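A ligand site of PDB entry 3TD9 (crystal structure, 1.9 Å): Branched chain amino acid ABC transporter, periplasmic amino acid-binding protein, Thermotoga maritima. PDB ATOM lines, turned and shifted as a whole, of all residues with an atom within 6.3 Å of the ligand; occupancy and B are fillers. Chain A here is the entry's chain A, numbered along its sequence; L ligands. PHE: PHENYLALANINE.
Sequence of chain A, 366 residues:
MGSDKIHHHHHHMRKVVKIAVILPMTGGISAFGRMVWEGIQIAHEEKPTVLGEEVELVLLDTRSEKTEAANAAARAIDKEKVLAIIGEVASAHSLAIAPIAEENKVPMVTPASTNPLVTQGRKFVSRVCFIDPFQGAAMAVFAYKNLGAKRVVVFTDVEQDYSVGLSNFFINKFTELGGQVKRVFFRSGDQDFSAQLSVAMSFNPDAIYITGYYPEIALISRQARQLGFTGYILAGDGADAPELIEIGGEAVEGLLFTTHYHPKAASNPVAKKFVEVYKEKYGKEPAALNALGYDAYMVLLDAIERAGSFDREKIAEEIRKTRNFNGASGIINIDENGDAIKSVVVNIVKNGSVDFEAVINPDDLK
The backbone NH (N) of Ser 91 sits at hydrogen-bond distance from an oxygen (OXT) of the ligand (3.0 Å).
An oxygen (O) of the ligand lies within hydrogen-bond range of the side-chain hydroxyl of Ser 91 (2.6 Å).
The side-chain carboxylate of Asp 237 lies within salt-bridge range of a nitrogen (N) of the ligand, 2.6 Å away.
The side-chain hydroxyl (OH) of Tyr 213 lies within hydrogen-bond range of an oxygen (OXT) of the ligand, 2.7 Å away.
The backbone carbonyl oxygen of Ala 112 is in hydrogen-bond range of a nitrogen (N) of the ligand, at 2.8 Å.
N of Thr 114 lies within hydrogen-bond range of O of the ligand (2.9 Å).
The side-chain hydroxyl (OG1) of Thr 114 is in hydrogen-bond range of a nitrogen (N) of the ligand (2.8 Å).
Residues that only touch the ligand: Phe 32, Val 89, Ala 90, Ser 113, Tyr 162, His 260 and Leu 289.
Hydrophobic or aromatic side chains within 4 Å of the ligand: Phe 32, Val 89, Ala 112, Tyr 162, Tyr 213, His 260 and Leu 289.
Of the 26 residues printed, 12 come within 4 Å of the ligand.
The nearest printed residue that does not touch the ligand is Gly 238 (4.2 Å).
N of Thr 114 sits at hydrogen-bond distance from OG of Ser 91, at 3.4 Å.
The side-chain hydroxyl (OG) of Ser 91 is in hydrogen-bond range of the backbone NH (N) of Asn 115.
OD1 of Asp 237 is in hydrogen-bond range of OH of Tyr 162 (2.5 Å).
OE1 of Gln 135 is in hydrogen-bond range of N of Asp 237.
OD2 of Asp 132 sits at hydrogen-bond distance from OG1 of Thr 114, 2.6 Å away.
O of Val 89 sits at hydrogen-bond distance from OG of Ser 113.
O of Ser 113 is in hydrogen-bond range of SG of Cys 129, 3.2 Å away.
The side-chain hydroxyl (OH) of Tyr 162 sits at hydrogen-bond distance from the backbone NH (N) of Gly 238 (3.2 Å).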
ATOM      1  N   PHE A  32       0.152  11.060 -10.927  1.00  0.00           N
ATOM      2  CA  PHE A  32      -0.720  10.460 -11.935  1.00  0.00           C
ATOM      3  C   PHE A  32      -1.207  11.460 -12.969  1.00  0.00           C
ATOM      4  O   PHE A  32      -1.194  11.158 -14.140  1.00  0.00           O
ATOM      5  CB  PHE A  32      -1.941   9.719 -11.298  1.00  0.00           C
ATOM      6  CG  PHE A  32      -1.583   8.507 -10.435  1.00  0.00           C
ATOM      7  CD1 PHE A  32      -0.383   7.818 -10.569  1.00  0.00           C
ATOM      8  CD2 PHE A  32      -2.463   8.080  -9.477  1.00  0.00           C
ATOM      9  CE1 PHE A  32      -0.114   6.715  -9.756  1.00  0.00           C
ATOM     10  CE2 PHE A  32      -2.181   7.003  -8.652  1.00  0.00           C
ATOM     11  CZ  PHE A  32      -1.025   6.316  -8.791  1.00  0.00           C
ATOM     12  N   VAL A  89      -8.126   9.268 -13.319  1.00  0.00           N
ATOM     13  CA  VAL A  89      -7.160   8.176 -13.133  1.00  0.00           C
ATOM     14  C   VAL A  89      -7.599   7.288 -11.990  1.00  0.00           C
ATOM     15  O   VAL A  89      -7.754   6.076 -12.192  1.00  0.00           O
ATOM     16  CB  VAL A  89      -5.712   8.689 -12.899  1.00  0.00           C
ATOM     17  CG1 VAL A  89      -4.760   7.508 -12.660  1.00  0.00           C
ATOM     18  CG2 VAL A  89      -5.264   9.491 -14.132  1.00  0.00           C
ATOM     19  N   ALA A  90      -7.789   7.869 -10.793  1.00  0.00           N
ATOM     20  CA  ALA A  90      -8.302   7.101  -9.660  1.00  0.00           C
ATOM     21  C   ALA A  90      -9.743   6.675  -9.923  1.00  0.00           C
ATOM     22  O   ALA A  90     -10.599   7.489 -10.279  1.00  0.00           O
ATOM     23  CB  ALA A  90      -8.207   7.903  -8.357  1.00  0.00           C
ATOM     24  N   SER A  91     -10.014   5.385  -9.736  1.00  0.00           N
ATOM     25  CA  SER A  91     -11.364   4.866  -9.920  1.00  0.00           C
ATOM     26  C   SER A  91     -12.409   5.610  -9.102  1.00  0.00           C
ATOM     27  O   SER A  91     -13.507   5.907  -9.609  1.00  0.00           O
ATOM     28  CB  SER A  91     -11.415   3.347  -9.666  1.00  0.00           C
ATOM     29  OG  SER A  91     -10.845   2.593 -10.738  1.00  0.00           O
ATOM     30  N   ALA A  92     -12.091   5.938  -7.847  1.00  0.00           N
ATOM     31  CA  ALA A  92     -13.013   6.760  -7.062  1.00  0.00           C
ATOM     32  C   ALA A  92     -13.388   8.042  -7.796  1.00  0.00           C
ATOM     33  O   ALA A  92     -14.539   8.436  -7.774  1.00  0.00           O
ATOM     34  CB  ALA A  92     -12.446   7.081  -5.684  1.00  0.00           C
ATOM     35  N   ALA A 112      -7.068   5.077 -17.456  1.00  0.00           N
ATOM     36  CA  ALA A 112      -6.370   4.274 -16.445  1.00  0.00           C
ATOM     37  C   ALA A 112      -7.209   3.739 -15.268  1.00  0.00           C
ATOM     38  O   ALA A 112      -6.672   2.956 -14.451  1.00  0.00           O
ATOM     39  CB  ALA A 112      -5.130   5.091 -15.895  1.00  0.00           C
ATOM     40  N   SER A 113      -8.464   4.160 -15.126  1.00  0.00           N
ATOM     41  CA  SER A 113      -9.336   3.575 -14.094  1.00  0.00           C
ATOM     42  C   SER A 113      -9.677   2.144 -14.454  1.00  0.00           C
ATOM     43  O   SER A 113     -10.109   1.841 -15.580  1.00  0.00           O
ATOM     44  CB  SER A 113     -10.576   4.425 -13.845  1.00  0.00           C
ATOM     45  OG  SER A 113     -10.194   5.710 -13.383  1.00  0.00           O
ATOM     46  N   THR A 114      -9.435   1.237 -13.492  1.00  0.00           N
ATOM     47  CA  THR A 114      -9.556  -0.186 -13.691  1.00  0.00           C
ATOM     48  C   THR A 114     -10.775  -0.817 -13.008  1.00  0.00           C
ATOM     49  O   THR A 114     -11.069  -1.975 -13.234  1.00  0.00           O
ATOM     50  CB  THR A 114      -8.256  -0.890 -13.254  1.00  0.00           C
ATOM     51  OG1 THR A 114      -7.878  -0.429 -11.937  1.00  0.00           O
ATOM     52  CG2 THR A 114      -7.165  -0.566 -14.263  1.00  0.00           C
ATOM     53  N   ASN A 115     -11.480  -0.084 -12.138  1.00  0.00           N
ATOM     54  CA  ASN A 115     -12.600  -0.670 -11.441  1.00  0.00           C
ATOM     55  C   ASN A 115     -13.753  -0.919 -12.427  1.00  0.00           C
ATOM     56  O   ASN A 115     -14.071  -0.030 -13.212  1.00  0.00           O
ATOM     57  CB  ASN A 115     -13.067   0.225 -10.281  1.00  0.00           C
ATOM     58  CG  ASN A 115     -14.140  -0.451  -9.415  1.00  0.00           C
ATOM     59  OD1 ASN A 115     -15.306  -0.506  -9.777  1.00  0.00           O
ATOM     60  ND2 ASN A 115     -13.736  -0.944  -8.271  1.00  0.00           N
ATOM     61  N   CYS A 129      -7.868   0.574 -20.885  1.00  0.00           N
ATOM     62  CA  CYS A 129      -7.074  -0.325 -20.044  1.00  0.00           C
ATOM     63  C   CYS A 129      -7.913  -1.523 -19.607  1.00  0.00           C
ATOM     64  O   CYS A 129      -9.122  -1.551 -19.828  1.00  0.00           O
ATOM     65  CB  CYS A 129      -6.527   0.426 -18.847  1.00  0.00           C
ATOM     66  SG  CYS A 129      -7.847   1.147 -17.748  1.00  0.00           S
ATOM     67  N   PHE A 130      -7.245  -2.527 -19.015  1.00  0.00           N
ATOM     68  CA  PHE A 130      -7.918  -3.665 -18.405  1.00  0.00           C
ATOM     69  C   PHE A 130      -8.762  -3.302 -17.198  1.00  0.00           C
ATOM     70  O   PHE A 130      -8.763  -2.149 -16.758  1.00  0.00           O
ATOM     71  CB  PHE A 130      -6.929  -4.783 -18.035  1.00  0.00           C
ATOM     72  CG  PHE A 130      -5.733  -4.357 -17.221  1.00  0.00           C
ATOM     73  CD1 PHE A 130      -5.857  -3.827 -15.939  1.00  0.00           C
ATOM     74  CD2 PHE A 130      -4.450  -4.512 -17.755  1.00  0.00           C
ATOM     75  CE1 PHE A 130      -4.731  -3.478 -15.191  1.00  0.00           C
ATOM     76  CE2 PHE A 130      -3.306  -4.170 -17.012  1.00  0.00           C
ATOM     77  CZ  PHE A 130      -3.444  -3.649 -15.726  1.00  0.00           C
ATOM     78  N   ASP A 132     -10.165  -4.748 -13.107  1.00  0.00           N
ATOM     79  CA  ASP A 132      -9.573  -5.344 -11.922  1.00  0.00           C
ATOM     80  C   ASP A 132      -9.833  -6.850 -11.590  1.00  0.00           C
ATOM     81  O   ASP A 132      -8.963  -7.484 -10.985  1.00  0.00           O
ATOM     82  CB  ASP A 132      -9.789  -4.425 -10.733  1.00  0.00           C
ATOM     83  CG  ASP A 132      -8.815  -3.208 -10.779  1.00  0.00           C
ATOM     84  OD1 ASP A 132      -7.709  -3.391 -11.309  1.00  0.00           O
ATOM     85  OD2 ASP A 132      -9.168  -2.097 -10.346  1.00  0.00           O
ATOM     86  N   GLN A 135      -6.754  -7.776 -13.284  1.00  0.00           N
ATOM     87  CA  GLN A 135      -5.559  -7.296 -12.571  1.00  0.00           C
ATOM     88  C   GLN A 135      -5.378  -8.030 -11.243  1.00  0.00           C
ATOM     89  O   GLN A 135      -4.280  -8.442 -10.948  1.00  0.00           O
ATOM     90  CB  GLN A 135      -5.538  -5.777 -12.353  1.00  0.00           C
ATOM     91  CG  GLN A 135      -4.188  -5.360 -11.758  1.00  0.00           C
ATOM     92  CD  GLN A 135      -3.948  -3.876 -11.541  1.00  0.00           C
ATOM     93  OE1 GLN A 135      -2.790  -3.491 -11.409  1.00  0.00           O
ATOM     94  NE2 GLN A 135      -5.007  -3.053 -11.509  1.00  0.00           N
ATOM     95  N   TYR A 162     -11.001   1.858  -5.933  1.00  0.00           N
ATOM     96  CA  TYR A 162     -10.038   1.034  -6.632  1.00  0.00           C
ATOM     97  C   TYR A 162      -9.438  -0.044  -5.735  1.00  0.00           C
ATOM     98  O   TYR A 162      -9.316  -1.214  -6.146  1.00  0.00           O
ATOM     99  CB  TYR A 162      -8.919   1.915  -7.156  1.00  0.00           C
ATOM    100  CG  TYR A 162      -7.638   1.230  -7.425  1.00  0.00           C
ATOM    101  CD1 TYR A 162      -7.504   0.374  -8.514  1.00  0.00           C
ATOM    102  CD2 TYR A 162      -6.515   1.476  -6.650  1.00  0.00           C
ATOM    103  CE1 TYR A 162      -6.305  -0.240  -8.784  1.00  0.00           C
ATOM    104  CE2 TYR A 162      -5.309   0.845  -6.908  1.00  0.00           C
ATOM    105  CZ  TYR A 162      -5.216  -0.009  -7.987  1.00  0.00           C
ATOM    106  OH  TYR A 162      -4.039  -0.625  -8.303  1.00  0.00           O
ATOM    107  N   SER A 163      -9.030   0.350  -4.544  1.00  0.00           N
ATOM    108  CA  SER A 163      -8.397  -0.532  -3.614  1.00  0.00           C
ATOM    109  C   SER A 163      -9.340  -1.599  -3.099  1.00  0.00           C
ATOM    110  O   SER A 163      -8.985  -2.768  -3.055  1.00  0.00           O
ATOM    111  CB  SER A 163      -7.751   0.238  -2.454  1.00  0.00           C
ATOM    112  OG  SER A 163      -7.144  -0.650  -1.533  1.00  0.00           O
ATOM    113  N   TYR A 213      -2.374   3.464  -3.335  1.00  0.00           N
ATOM    114  CA  TYR A 213      -1.553   4.291  -4.262  1.00  0.00           C
ATOM    115  C   TYR A 213      -0.156   4.513  -3.689  1.00  0.00           C
ATOM    116  O   TYR A 213       0.086   4.231  -2.524  1.00  0.00           O
ATOM    117  CB  TYR A 213      -2.233   5.617  -4.590  1.00  0.00           C
ATOM    118  CG  TYR A 213      -3.578   5.467  -5.254  1.00  0.00           C
ATOM    119  CD1 TYR A 213      -3.711   4.745  -6.394  1.00  0.00           C
ATOM    120  CD2 TYR A 213      -4.714   6.045  -4.708  1.00  0.00           C
ATOM    121  CE1 TYR A 213      -4.914   4.558  -7.004  1.00  0.00           C
ATOM    122  CE2 TYR A 213      -5.968   5.884  -5.343  1.00  0.00           C
ATOM    123  CZ  TYR A 213      -6.060   5.116  -6.464  1.00  0.00           C
ATOM    124  OH  TYR A 213      -7.244   4.925  -7.129  1.00  0.00           O
ATOM    125  N   ASP A 237      -1.283  -1.470  -9.819  1.00  0.00           N
ATOM    126  CA  ASP A 237      -0.868  -0.370 -10.690  1.00  0.00           C
ATOM    127  C   ASP A 237      -0.757   0.958  -9.953  1.00  0.00           C
ATOM    128  O   ASP A 237      -0.056   1.846 -10.379  1.00  0.00           O
ATOM    129  CB  ASP A 237      -1.700  -0.321 -12.013  1.00  0.00           C
ATOM    130  CG  ASP A 237      -3.212  -0.068 -11.816  1.00  0.00           C
ATOM    131  OD1 ASP A 237      -3.755  -0.270 -10.728  1.00  0.00           O
ATOM    132  OD2 ASP A 237      -3.864   0.289 -12.833  1.00  0.00           O
ATOM    133  N   GLY A 238      -1.384   1.033  -8.774  1.00  0.00           N
ATOM    134  CA  GLY A 238      -1.226   2.185  -7.907  1.00  0.00           C
ATOM    135  C   GLY A 238       0.182   2.481  -7.508  1.00  0.00           C
ATOM    136  O   GLY A 238       0.483   3.600  -7.140  1.00  0.00           O
ATOM    137  N   ALA A 239       1.061   1.473  -7.597  1.00  0.00           N
ATOM    138  CA  ALA A 239       2.474   1.621  -7.334  1.00  0.00           C
ATOM    139  C   ALA A 239       3.225   2.373  -8.421  1.00  0.00           C
ATOM    140  O   ALA A 239       4.339   2.782  -8.192  1.00  0.00           O
ATOM    141  CB  ALA A 239       3.104   0.242  -7.170  1.00  0.00           C
ATOM    142  N   ASP A 240       2.628   2.512  -9.616  1.00  0.00           N
ATOM    143  CA  ASP A 240       3.417   2.796 -10.838  1.00  0.00           C
ATOM    144  C   ASP A 240       3.628   4.290 -11.079  1.00  0.00           C
ATOM    145  O   ASP A 240       3.062   4.865 -11.980  1.00  0.00           O
ATOM    146  CB  ASP A 240       2.764   2.131 -12.067  1.00  0.00           C
ATOM    147  CG  ASP A 240       3.717   2.002 -13.235  1.00  0.00           C
ATOM    148  OD1 ASP A 240       4.920   2.281 -13.058  1.00  0.00           O
ATOM    149  OD2 ASP A 240       3.269   1.599 -14.345  1.00  0.00           O
ATOM    150  N   ALA A 241       4.437   4.905 -10.215  1.00  0.00           N
ATOM    151  CA  ALA A 241       4.871   6.310 -10.343  1.00  0.00           C
ATOM    152  C   ALA A 241       6.324   6.273  -9.875  1.00  0.00           C
ATOM    153  O   ALA A 241       6.632   5.527  -8.962  1.00  0.00           O
ATOM    154  CB  ALA A 241       4.058   7.205  -9.422  1.00  0.00           C
ATOM    155  N   THR A 259       1.015  -3.773 -13.694  1.00  0.00           N
ATOM    156  CA  THR A 259       0.694  -2.541 -14.398  1.00  0.00           C
ATOM    157  C   THR A 259       0.333  -2.888 -15.839  1.00  0.00           C
ATOM    158  O   THR A 259       0.028  -4.054 -16.143  1.00  0.00           O
ATOM    159  CB  THR A 259       1.849  -1.482 -14.251  1.00  0.00           C
ATOM    160  OG1 THR A 259       1.449  -0.241 -14.834  1.00  0.00           O
ATOM    161  CG2 THR A 259       3.207  -2.017 -14.876  1.00  0.00           C
ATOM    162  N   HIS A 260       0.381  -1.870 -16.714  1.00  0.00           N
ATOM    163  CA  HIS A 260      -0.214  -1.923 -18.029  1.00  0.00           C
ATOM    164  C   HIS A 260       0.822  -2.026 -19.121  1.00  0.00           C
ATOM    165  O   HIS A 260       0.450  -2.209 -20.252  1.00  0.00           O
ATOM    166  CB  HIS A 260      -1.016  -0.635 -18.286  1.00  0.00           C
ATOM    167  CG  HIS A 260      -2.064  -0.364 -17.259  1.00  0.00           C
ATOM    168  ND1 HIS A 260      -3.411  -0.558 -17.488  1.00  0.00           N
ATOM    169  CD2 HIS A 260      -1.971   0.079 -15.985  1.00  0.00           C
ATOM    170  CE1 HIS A 260      -4.097  -0.222 -16.406  1.00  0.00           C
ATOM    171  NE2 HIS A 260      -3.247   0.160 -15.477  1.00  0.00           N
ATOM    172  N   ALA A 288       3.520   3.634 -17.923  1.00  0.00           N
ATOM    173  CA  ALA A 288       2.201   3.187 -18.338  1.00  0.00           C
ATOM    174  C   ALA A 288       1.255   4.371 -18.506  1.00  0.00           C
ATOM    175  O   ALA A 288       0.569   4.506 -19.513  1.00  0.00           O
ATOM    176  CB  ALA A 288       1.621   2.203 -17.289  1.00  0.00           C
ATOM    177  N   LEU A 289       1.225   5.239 -17.514  1.00  0.00           N
ATOM    178  CA  LEU A 289       0.273   6.335 -17.559  1.00  0.00           C
ATOM    179  C   LEU A 289       0.603   7.345 -18.673  1.00  0.00           C
ATOM    180  O   LEU A 289      -0.300   7.944 -19.219  1.00  0.00           O
ATOM    181  CB  LEU A 289       0.186   7.039 -16.194  1.00  0.00           C
ATOM    182  CG  LEU A 289      -0.544   6.336 -15.060  1.00  0.00           C
ATOM    183  CD1 LEU A 289      -0.467   7.189 -13.781  1.00  0.00           C
ATOM    184  CD2 LEU A 289      -1.999   6.168 -15.415  1.00  0.00           C
ATOM    185  N   LEU A 292      -0.842   5.481 -21.704  1.00  0.00           N
ATOM    186  CA  LEU A 292      -2.295   5.394 -21.550  1.00  0.00           C
ATOM    187  C   LEU A 292      -2.982   6.757 -21.832  1.00  0.00           C
ATOM    188  O   LEU A 292      -4.020   6.785 -22.454  1.00  0.00           O
ATOM    189  CB  LEU A 292      -2.636   4.859 -20.154  1.00  0.00           C
ATOM    190  CG  LEU A 292      -2.377   3.385 -19.884  1.00  0.00           C
ATOM    191  CD1 LEU A 292      -2.584   3.108 -18.382  1.00  0.00           C
ATOM    192  CD2 LEU A 292      -3.254   2.459 -20.674  1.00  0.00           C
HETATM  193  N   PHE L   1      -5.962   1.673 -12.053  1.00  0.00           N
HETATM  194  CA  PHE L   1      -5.905   2.690 -10.954  1.00  0.00           C
HETATM  195  C   PHE L   1      -7.333   3.020 -10.499  1.00  0.00           C
HETATM  196  O   PHE L   1      -8.288   2.577 -11.158  1.00  0.00           O
HETATM  197  CB  PHE L   1      -5.248   4.011 -11.440  1.00  0.00           C
HETATM  198  CG  PHE L   1      -3.852   3.860 -11.928  1.00  0.00           C
HETATM  199  CD1 PHE L   1      -3.590   3.293 -13.171  1.00  0.00           C
HETATM  200  CD2 PHE L   1      -2.799   4.361 -11.189  1.00  0.00           C
HETATM  201  CE1 PHE L   1      -2.281   3.163 -13.638  1.00  0.00           C
HETATM  202  CE2 PHE L   1      -1.498   4.214 -11.618  1.00  0.00           C
HETATM  203  CZ  PHE L   1      -1.227   3.620 -12.870  1.00  0.00           C
HETATM  204  OXT PHE L   1      -7.539   3.774  -9.527  1.00  0.00           O
